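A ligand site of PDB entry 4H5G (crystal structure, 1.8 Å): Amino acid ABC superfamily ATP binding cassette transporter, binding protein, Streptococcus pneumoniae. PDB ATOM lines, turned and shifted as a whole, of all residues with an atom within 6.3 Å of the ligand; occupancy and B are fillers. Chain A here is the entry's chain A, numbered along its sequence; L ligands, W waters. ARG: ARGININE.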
ATOM      1  N   THR A  18      -4.317 -22.649 -14.194  1.00  0.00           N
ATOM      2  CA  THR A  18      -4.849 -23.560 -15.216  1.00  0.00           C
ATOM      3  C   THR A  18      -6.266 -23.156 -15.600  1.00  0.00           C
ATOM      4  O   THR A  18      -6.879 -22.306 -14.956  1.00  0.00           O
ATOM      5  CB  THR A  18      -4.833 -25.037 -14.763  1.00  0.00           C
ATOM      6  OG1 THR A  18      -4.928 -25.883 -15.912  1.00  0.00           O
ATOM      7  CG2 THR A  18      -6.002 -25.366 -13.834  1.00  0.00           C
ATOM      8  N   SER A  19      -6.794 -23.796 -16.639  1.00  0.00           N
ATOM      9  CA  SER A  19      -8.152 -23.551 -17.107  1.00  0.00           C
ATOM     10  C   SER A  19      -8.861 -24.894 -17.231  1.00  0.00           C
ATOM     11  O   SER A  19      -8.687 -25.602 -18.221  1.00  0.00           O
ATOM     12  CB  SER A  19      -8.136 -22.828 -18.464  1.00  0.00           C
ATOM     13  OG  SER A  19      -9.407 -22.776 -19.087  1.00  0.00           O
ATOM     14  N   PRO A  20      -9.662 -25.268 -16.213  1.00  0.00           N
ATOM     15  CA  PRO A  20     -10.235 -26.618 -16.172  1.00  0.00           C
ATOM     16  C   PRO A  20     -11.460 -26.817 -17.063  1.00  0.00           C
ATOM     17  O   PRO A  20     -12.532 -27.183 -16.561  1.00  0.00           O
ATOM     18  CB  PRO A  20     -10.593 -26.792 -14.701  1.00  0.00           C
ATOM     19  CG  PRO A  20     -10.930 -25.410 -14.250  1.00  0.00           C
ATOM     20  CD  PRO A  20     -10.009 -24.487 -15.015  1.00  0.00           C
ATOM     21  N   ASP A  21     -11.302 -26.589 -18.367  1.00  0.00           N
ATOM     22  CA  ASP A  21     -12.381 -26.806 -19.341  1.00  0.00           C
ATOM     23  C   ASP A  21     -11.880 -27.689 -20.481  1.00  0.00           C
ATOM     24  O   ASP A  21     -12.318 -27.551 -21.615  1.00  0.00           O
ATOM     25  CB  ASP A  21     -12.857 -25.462 -19.925  1.00  0.00           C
ATOM     26  CG  ASP A  21     -11.747 -24.701 -20.659  1.00  0.00           C
ATOM     27  OD1 ASP A  21     -10.572 -25.067 -20.495  1.00  0.00           O
ATOM     28  OD2 ASP A  21     -12.052 -23.714 -21.375  1.00  0.00           O
ATOM     29  N   TYR A  22     -10.993 -28.630 -20.165  1.00  0.00           N
ATOM     30  CA  TYR A  22     -10.179 -29.232 -21.229  1.00  0.00           C
ATOM     31  C   TYR A  22      -9.790 -30.676 -20.905  1.00  0.00           C
ATOM     32  O   TYR A  22      -8.602 -31.006 -20.886  1.00  0.00           O
ATOM     33  CB  TYR A  22      -8.926 -28.351 -21.429  1.00  0.00           C
ATOM     34  CG  TYR A  22      -8.503 -28.127 -22.884  1.00  0.00           C
ATOM     35  CD1 TYR A  22      -9.414 -27.672 -23.829  1.00  0.00           C
ATOM     36  CD2 TYR A  22      -7.194 -28.327 -23.289  1.00  0.00           C
ATOM     37  CE1 TYR A  22      -9.040 -27.433 -25.162  1.00  0.00           C
ATOM     38  CE2 TYR A  22      -6.796 -28.106 -24.622  1.00  0.00           C
ATOM     39  CZ  TYR A  22      -7.735 -27.660 -25.544  1.00  0.00           C
ATOM     40  OH  TYR A  22      -7.364 -27.430 -26.855  1.00  0.00           O
ATOM     41  N   PHE A  25      -6.810 -33.060 -20.066  1.00  0.00           N
ATOM     42  CA  PHE A  25      -5.687 -32.309 -19.495  1.00  0.00           C
ATOM     43  C   PHE A  25      -6.039 -31.742 -18.114  1.00  0.00           C
ATOM     44  O   PHE A  25      -5.324 -31.943 -17.142  1.00  0.00           O
ATOM     45  CB  PHE A  25      -5.261 -31.172 -20.426  1.00  0.00           C
ATOM     46  CG  PHE A  25      -4.624 -31.636 -21.711  1.00  0.00           C
ATOM     47  CD1 PHE A  25      -3.294 -32.043 -21.721  1.00  0.00           C
ATOM     48  CD2 PHE A  25      -5.336 -31.651 -22.889  1.00  0.00           C
ATOM     49  CE1 PHE A  25      -2.708 -32.469 -22.893  1.00  0.00           C
ATOM     50  CE2 PHE A  25      -4.741 -32.071 -24.062  1.00  0.00           C
ATOM     51  CZ  PHE A  25      -3.423 -32.477 -24.064  1.00  0.00           C
ATOM     52  N   GLU A  26      -7.131 -30.995 -18.063  1.00  0.00           N
ATOM     53  CA  GLU A  26      -7.677 -30.507 -16.783  1.00  0.00           C
ATOM     54  C   GLU A  26      -9.167 -30.258 -16.927  1.00  0.00           C
ATOM     55  O   GLU A  26      -9.640 -29.735 -17.942  1.00  0.00           O
ATOM     56  CB  GLU A  26      -6.979 -29.217 -16.322  1.00  0.00           C
ATOM     57  CG  GLU A  26      -6.887 -28.130 -17.379  1.00  0.00           C
ATOM     58  CD  GLU A  26      -5.606 -28.221 -18.179  1.00  0.00           C
ATOM     59  OE1 GLU A  26      -4.585 -28.670 -17.608  1.00  0.00           O
ATOM     60  OE2 GLU A  26      -5.615 -27.869 -19.378  1.00  0.00           O
ATOM     61  N   ASP A  41      -2.691 -32.985 -16.467  1.00  0.00           N
ATOM     62  CA  ASP A  41      -1.876 -31.817 -16.109  1.00  0.00           C
ATOM     63  C   ASP A  41      -1.831 -31.629 -14.591  1.00  0.00           C
ATOM     64  O   ASP A  41      -0.826 -31.164 -14.048  1.00  0.00           O
ATOM     65  CB  ASP A  41      -2.438 -30.528 -16.729  1.00  0.00           C
ATOM     66  CG  ASP A  41      -1.918 -30.265 -18.140  1.00  0.00           C
ATOM     67  OD1 ASP A  41      -1.002 -30.973 -18.612  1.00  0.00           O
ATOM     68  OD2 ASP A  41      -2.402 -29.305 -18.763  1.00  0.00           O
ATOM     69  N   PHE A  63      -8.821 -19.728 -19.993  1.00  0.00           N
ATOM     70  CA  PHE A  63      -7.523 -19.936 -20.617  1.00  0.00           C
ATOM     71  C   PHE A  63      -6.824 -18.635 -20.987  1.00  0.00           C
ATOM     72  O   PHE A  63      -5.621 -18.501 -20.763  1.00  0.00           O
ATOM     73  CB  PHE A  63      -7.579 -20.850 -21.827  1.00  0.00           C
ATOM     74  CG  PHE A  63      -6.209 -21.128 -22.407  1.00  0.00           C
ATOM     75  CD1 PHE A  63      -5.393 -22.096 -21.852  1.00  0.00           C
ATOM     76  CD2 PHE A  63      -5.710 -20.360 -23.452  1.00  0.00           C
ATOM     77  CE1 PHE A  63      -4.125 -22.336 -22.359  1.00  0.00           C
ATOM     78  CE2 PHE A  63      -4.437 -20.571 -23.954  1.00  0.00           C
ATOM     79  CZ  PHE A  63      -3.655 -21.561 -23.411  1.00  0.00           C
ATOM     80  N   VAL A  79       0.103 -24.396 -16.235  1.00  0.00           N
ATOM     81  CA  VAL A  79       0.019 -25.734 -16.843  1.00  0.00           C
ATOM     82  C   VAL A  79      -1.418 -25.885 -17.304  1.00  0.00           C
ATOM     83  O   VAL A  79      -2.336 -25.989 -16.498  1.00  0.00           O
ATOM     84  CB  VAL A  79       0.350 -26.837 -15.829  1.00  0.00           C
ATOM     85  CG1 VAL A  79       0.377 -28.208 -16.524  1.00  0.00           C
ATOM     86  CG2 VAL A  79       1.722 -26.594 -15.151  1.00  0.00           C
ATOM     87  N   ALA A  80      -1.609 -25.856 -18.618  1.00  0.00           N
ATOM     88  CA  ALA A  80      -2.973 -25.853 -19.156  1.00  0.00           C
ATOM     89  C   ALA A  80      -2.995 -26.310 -20.601  1.00  0.00           C
ATOM     90  O   ALA A  80      -3.633 -25.676 -21.453  1.00  0.00           O
ATOM     91  CB  ALA A  80      -3.578 -24.447 -19.044  1.00  0.00           C
ATOM     92  N   GLY A  81      -2.291 -27.407 -20.878  1.00  0.00           N
ATOM     93  CA  GLY A  81      -2.186 -27.888 -22.263  1.00  0.00           C
ATOM     94  C   GLY A  81      -1.634 -26.795 -23.160  1.00  0.00           C
ATOM     95  O   GLY A  81      -2.111 -26.573 -24.276  1.00  0.00           O
ATOM     96  N   ILE A  82      -0.611 -26.119 -22.658  1.00  0.00           N
ATOM     97  CA  ILE A  82      -0.123 -24.897 -23.313  1.00  0.00           C
ATOM     98  C   ILE A  82       0.913 -25.215 -24.381  1.00  0.00           C
ATOM     99  O   ILE A  82       1.988 -25.740 -24.062  1.00  0.00           O
ATOM    100  CB  ILE A  82       0.521 -23.957 -22.290  1.00  0.00           C
ATOM    101  CG1 ILE A  82      -0.504 -23.564 -21.212  1.00  0.00           C
ATOM    102  CG2 ILE A  82       1.115 -22.719 -22.977  1.00  0.00           C
ATOM    103  CD1 ILE A  82       0.097 -22.780 -20.036  1.00  0.00           C
ATOM    104  N   SER A  83       0.609 -24.870 -25.625  1.00  0.00           N
ATOM    105  CA  SER A  83       1.557 -25.018 -26.736  1.00  0.00           C
ATOM    106  C   SER A  83       2.764 -24.092 -26.548  1.00  0.00           C
ATOM    107  O   SER A  83       2.622 -22.883 -26.391  1.00  0.00           O
ATOM    108  CB  SER A  83       0.861 -24.683 -28.056  1.00  0.00           C
ATOM    109  OG  SER A  83      -0.249 -25.523 -28.289  1.00  0.00           O
ATOM    110  N   ALA A  84       3.971 -24.649 -26.615  1.00  0.00           N
ATOM    111  CA  ALA A  84       5.188 -23.835 -26.448  1.00  0.00           C
ATOM    112  C   ALA A  84       5.579 -23.173 -27.773  1.00  0.00           C
ATOM    113  O   ALA A  84       6.543 -23.571 -28.437  1.00  0.00           O
ATOM    114  CB  ALA A  84       6.326 -24.673 -25.893  1.00  0.00           C
ATOM    115  N   THR A  85       4.846 -22.128 -28.152  1.00  0.00           N
ATOM    116  CA  THR A  85       5.079 -21.456 -29.436  1.00  0.00           C
ATOM    117  C   THR A  85       6.262 -20.493 -29.398  1.00  0.00           C
ATOM    118  O   THR A  85       6.664 -20.026 -28.336  1.00  0.00           O
ATOM    119  CB  THR A  85       3.829 -20.670 -29.871  1.00  0.00           C
ATOM    120  OG1 THR A  85       3.658 -19.551 -28.984  1.00  0.00           O
ATOM    121  CG2 THR A  85       2.579 -21.554 -29.812  1.00  0.00           C
ATOM    122  N   ARG A  88       5.201 -17.245 -27.803  1.00  0.00           N
ATOM    123  CA  ARG A  88       5.113 -17.304 -26.343  1.00  0.00           C
ATOM    124  C   ARG A  88       6.485 -17.382 -25.701  1.00  0.00           C
ATOM    125  O   ARG A  88       6.689 -16.898 -24.598  1.00  0.00           O
ATOM    126  CB  ARG A  88       4.227 -18.471 -25.918  1.00  0.00           C
ATOM    127  CG  ARG A  88       2.738 -18.201 -26.170  1.00  0.00           C
ATOM    128  CD  ARG A  88       1.939 -19.465 -26.033  1.00  0.00           C
ATOM    129  NE  ARG A  88       0.506 -19.215 -26.208  1.00  0.00           N
ATOM    130  CZ  ARG A  88      -0.408 -20.174 -26.256  1.00  0.00           C
ATOM    131  NH1 ARG A  88      -0.022 -21.436 -26.163  1.00  0.00           N
ATOM    132  NH2 ARG A  88      -1.695 -19.871 -26.404  1.00  0.00           N
ATOM    133  N   ILE A 103      -4.041 -31.369 -33.688  1.00  0.00           N
ATOM    134  CA  ILE A 103      -5.166 -30.477 -33.468  1.00  0.00           C
ATOM    135  C   ILE A 103      -6.285 -30.888 -34.429  1.00  0.00           C
ATOM    136  O   ILE A 103      -6.037 -31.194 -35.596  1.00  0.00           O
ATOM    137  CB  ILE A 103      -4.732 -29.021 -33.667  1.00  0.00           C
ATOM    138  CG1 ILE A 103      -3.511 -28.740 -32.780  1.00  0.00           C
ATOM    139  CG2 ILE A 103      -5.897 -28.076 -33.385  1.00  0.00           C
ATOM    140  CD1 ILE A 103      -2.922 -27.366 -32.881  1.00  0.00           C
ATOM    141  N   GLN A 129     -11.171 -21.379 -29.154  1.00  0.00           N
ATOM    142  CA  GLN A 129     -11.031 -20.734 -27.838  1.00  0.00           C
ATOM    143  C   GLN A 129     -10.170 -19.487 -27.927  1.00  0.00           C
ATOM    144  O   GLN A 129      -9.108 -19.493 -28.555  1.00  0.00           O
ATOM    145  CB  GLN A 129     -10.422 -21.734 -26.849  1.00  0.00           C
ATOM    146  CG  GLN A 129     -10.300 -21.214 -25.425  1.00  0.00           C
ATOM    147  CD  GLN A 129     -10.106 -22.347 -24.440  1.00  0.00           C
ATOM    148  OE1 GLN A 129      -9.405 -23.329 -24.724  1.00  0.00           O
ATOM    149  NE2 GLN A 129     -10.714 -22.221 -23.262  1.00  0.00           N
ATOM    150  N   GLY A 131      -7.505 -16.747 -27.417  1.00  0.00           N
ATOM    151  CA  GLY A 131      -6.139 -16.726 -26.959  1.00  0.00           C
ATOM    152  C   GLY A 131      -5.369 -18.016 -27.212  1.00  0.00           C
ATOM    153  O   GLY A 131      -4.356 -18.240 -26.577  1.00  0.00           O
ATOM    154  N   THR A 132      -5.841 -18.843 -28.150  1.00  0.00           N
ATOM    155  CA  THR A 132      -5.231 -20.157 -28.360  1.00  0.00           C
ATOM    156  C   THR A 132      -4.640 -20.394 -29.750  1.00  0.00           C
ATOM    157  O   THR A 132      -4.963 -19.689 -30.710  1.00  0.00           O
ATOM    158  CB  THR A 132      -6.205 -21.335 -28.073  1.00  0.00           C
ATOM    159  OG1 THR A 132      -7.203 -21.385 -29.103  1.00  0.00           O
ATOM    160  CG2 THR A 132      -6.867 -21.211 -26.688  1.00  0.00           C
ATOM    161  N   VAL A 133      -3.791 -21.416 -29.831  1.00  0.00           N
ATOM    162  CA  VAL A 133      -3.238 -21.876 -31.106  1.00  0.00           C
ATOM    163  C   VAL A 133      -4.325 -22.359 -32.085  1.00  0.00           C
ATOM    164  O   VAL A 133      -4.321 -21.947 -33.245  1.00  0.00           O
ATOM    165  CB  VAL A 133      -2.094 -22.915 -30.900  1.00  0.00           C
ATOM    166  CG1 VAL A 133      -1.654 -23.542 -32.238  1.00  0.00           C
ATOM    167  CG2 VAL A 133      -0.918 -22.251 -30.191  1.00  0.00           C
ATOM    168  N   PRO A 134      -5.266 -23.215 -31.642  1.00  0.00           N
ATOM    169  CA  PRO A 134      -6.339 -23.604 -32.584  1.00  0.00           C
ATOM    170  C   PRO A 134      -7.132 -22.410 -33.118  1.00  0.00           C
ATOM    171  O   PRO A 134      -7.590 -22.445 -34.262  1.00  0.00           O
ATOM    172  CB  PRO A 134      -7.240 -24.511 -31.735  1.00  0.00           C
ATOM    173  CG  PRO A 134      -6.312 -25.096 -30.720  1.00  0.00           C
ATOM    174  CD  PRO A 134      -5.344 -23.982 -30.379  1.00  0.00           C
ATOM    175  N   MET A 153     -14.061 -23.432 -23.346  1.00  0.00           N
ATOM    176  CA  MET A 153     -14.240 -24.534 -24.312  1.00  0.00           C
ATOM    177  C   MET A 153     -15.581 -25.246 -24.154  1.00  0.00           C
ATOM    178  O   MET A 153     -16.163 -25.684 -25.148  1.00  0.00           O
ATOM    179  CB  MET A 153     -13.087 -25.548 -24.228  1.00  0.00           C
ATOM    180  CG  MET A 153     -13.237 -26.717 -25.235  1.00  0.00           C
ATOM    181  SD  MET A 153     -13.405 -26.159 -26.943  1.00  0.00           S
ATOM    182  CE  MET A 153     -11.758 -25.534 -27.242  1.00  0.00           C
ATOM    183  N   ASP A 171      -7.391 -29.130 -29.265  1.00  0.00           N
ATOM    184  CA  ASP A 171      -6.367 -30.185 -29.209  1.00  0.00           C
ATOM    185  C   ASP A 171      -7.026 -31.556 -29.368  1.00  0.00           C
ATOM    186  O   ASP A 171      -8.082 -31.809 -28.803  1.00  0.00           O
ATOM    187  CB  ASP A 171      -5.582 -30.101 -27.896  1.00  0.00           C
ATOM    188  CG  ASP A 171      -4.592 -28.953 -27.899  1.00  0.00           C
ATOM    189  OD1 ASP A 171      -3.504 -29.125 -28.474  1.00  0.00           O
ATOM    190  OD2 ASP A 171      -4.928 -27.862 -27.380  1.00  0.00           O
ATOM    191  N   ASN A 200       2.931 -29.485 -25.913  1.00  0.00           N
ATOM    192  CA  ASN A 200       2.559 -28.934 -24.614  1.00  0.00           C
ATOM    193  C   ASN A 200       3.758 -28.834 -23.673  1.00  0.00           C
ATOM    194  O   ASN A 200       4.531 -29.771 -23.565  1.00  0.00           O
ATOM    195  CB  ASN A 200       1.501 -29.824 -23.966  1.00  0.00           C
ATOM    196  CG  ASN A 200       0.287 -29.964 -24.834  1.00  0.00           C
ATOM    197  OD1 ASN A 200      -0.476 -29.015 -25.007  1.00  0.00           O
ATOM    198  ND2 ASN A 200       0.117 -31.147 -25.428  1.00  0.00           N
HETATM  199  N   ARG L   1      -2.913 -25.908 -26.840  1.00  0.00           N
HETATM  200  CA  ARG L   1      -3.662 -24.676 -27.108  1.00  0.00           C
HETATM  201  C   ARG L   1      -2.847 -23.450 -26.747  1.00  0.00           C
HETATM  202  O   ARG L   1      -1.864 -23.520 -25.993  1.00  0.00           O
HETATM  203  CB  ARG L   1      -4.996 -24.654 -26.344  1.00  0.00           C
HETATM  204  CG  ARG L   1      -4.881 -24.951 -24.848  1.00  0.00           C
HETATM  205  CD  ARG L   1      -6.214 -24.695 -24.127  1.00  0.00           C
HETATM  206  NE  ARG L   1      -6.162 -25.146 -22.725  1.00  0.00           N
HETATM  207  CZ  ARG L   1      -7.182 -25.104 -21.874  1.00  0.00           C
HETATM  208  NH1 ARG L   1      -7.033 -25.541 -20.626  1.00  0.00           N
HETATM  209  NH2 ARG L   1      -8.350 -24.609 -22.273  1.00  0.00           N
HETATM  210  OXT ARG L   1      -3.159 -22.348 -27.209  1.00  0.00           O
HETATM  211  O   HOH W   1      -2.826 -26.393 -29.741  1.00  0.00           O
HETATM  212  O   HOH W   2      -0.938 -28.644 -27.764  1.00  0.00           O
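O of Gly 81 sits at hydrogen-bond distance from N of the ligand.
The guanidinium group (NH1) of Arg 88 lies within salt-bridge range of an oxygen (O) of the ligand (2.8 Å).
The backbone NH (N) of Ser 83 sits at hydrogen-bond distance from an oxygen (O) of the ligand (2.8 Å).
OG of Ser 83 lies within hydrogen-bond range of N of the ligand (3.1 Å).
OXT of the ligand is in hydrogen-bond range of N of Val 133 (2.9 Å).
OD2 of Asp 171 lies within salt-bridge range of N of the ligand (2.9 Å).
The backbone carbonyl oxygen of Ala 80 sits at hydrogen-bond distance from a nitrogen (NE) of the ligand, at 2.9 Å.
OD1 of Asp 21 lies within salt-bridge range of NH2 of the ligand (2.9 Å).
The backbone carbonyl oxygen of Ser 19 sits at hydrogen-bond distance from a nitrogen (NH1) of the ligand (2.9 Å).
A nitrogen (NH2) of the ligand lies within hydrogen-bond range of the side-chain amide oxygen (OE1) of Gln 129 (3.0 Å).
OE2 of Glu 26 is in salt-bridge range of NH1 of the ligand (3.0 Å).
O of Gly 81 sits close to OD1 of Asn 200.
N of Gly 81 is in hydrogen-bond range of OD2 of Asp 41 (2.8 Å).
NH1 of Arg 88 sits at hydrogen-bond distance from O of Ser 83 (3.0 Å).
The side-chain hydroxyl (OG1) of Thr 85 sits at hydrogen-bond distance from the backbone NH (N) of Arg 88, at 3.0 Å.
The side-chain carboxylate (OD1) of Asp 21 is in hydrogen-bond range of the side-chain hydroxyl (OG) of Ser 19 (2.9 Å).
NE2 of Gln 129 lies within hydrogen-bond range of OD2 of Asp 21 (2.8 Å).
The backbone NH (N) of Met 153 lies within hydrogen-bond range of the side-chain carboxylate (OD2) of Asp 21.
The side-chain carboxylate of Glu 26 sits at hydrogen-bond distance from the side-chain hydroxyl of Thr 18, at 3.3 Å.
Tyr 22 touches the ligand (CD2 to NE, 3.4 Å).
Phe 63 touches the ligand.
CA of Ile 82 touches O of the ligand, at 3.5 Å.
Thr 132 touches the ligand (CA to OXT, 3.2 Å).
Pro 134 touches the ligand.
Hydrophobic or aromatic side chains within 4 Å of the ligand: Tyr 22, Phe 63, Ala 80, Val 133 and Pro 134.
Within 4 Å of the ligand: Ser 19, Asp 21, Tyr 22, Glu 26, Phe 63, Ala 80, Gly 81, Ile 82, Ser 83, Arg 88, Gln 129, Thr 132, Val 133, Pro 134 and Asp 171.
Water W1 lies within hydrogen-bond range of N of the ligand (2.9 Å), OG of Ser 83 (3.1 Å) and OD1 of Asp 171 (3.1 Å).
Water W2 lies within hydrogen-bond range of OD1 of Asp 171, OD1 of Asn 200, OG of Ser 83 and N of the ligand.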
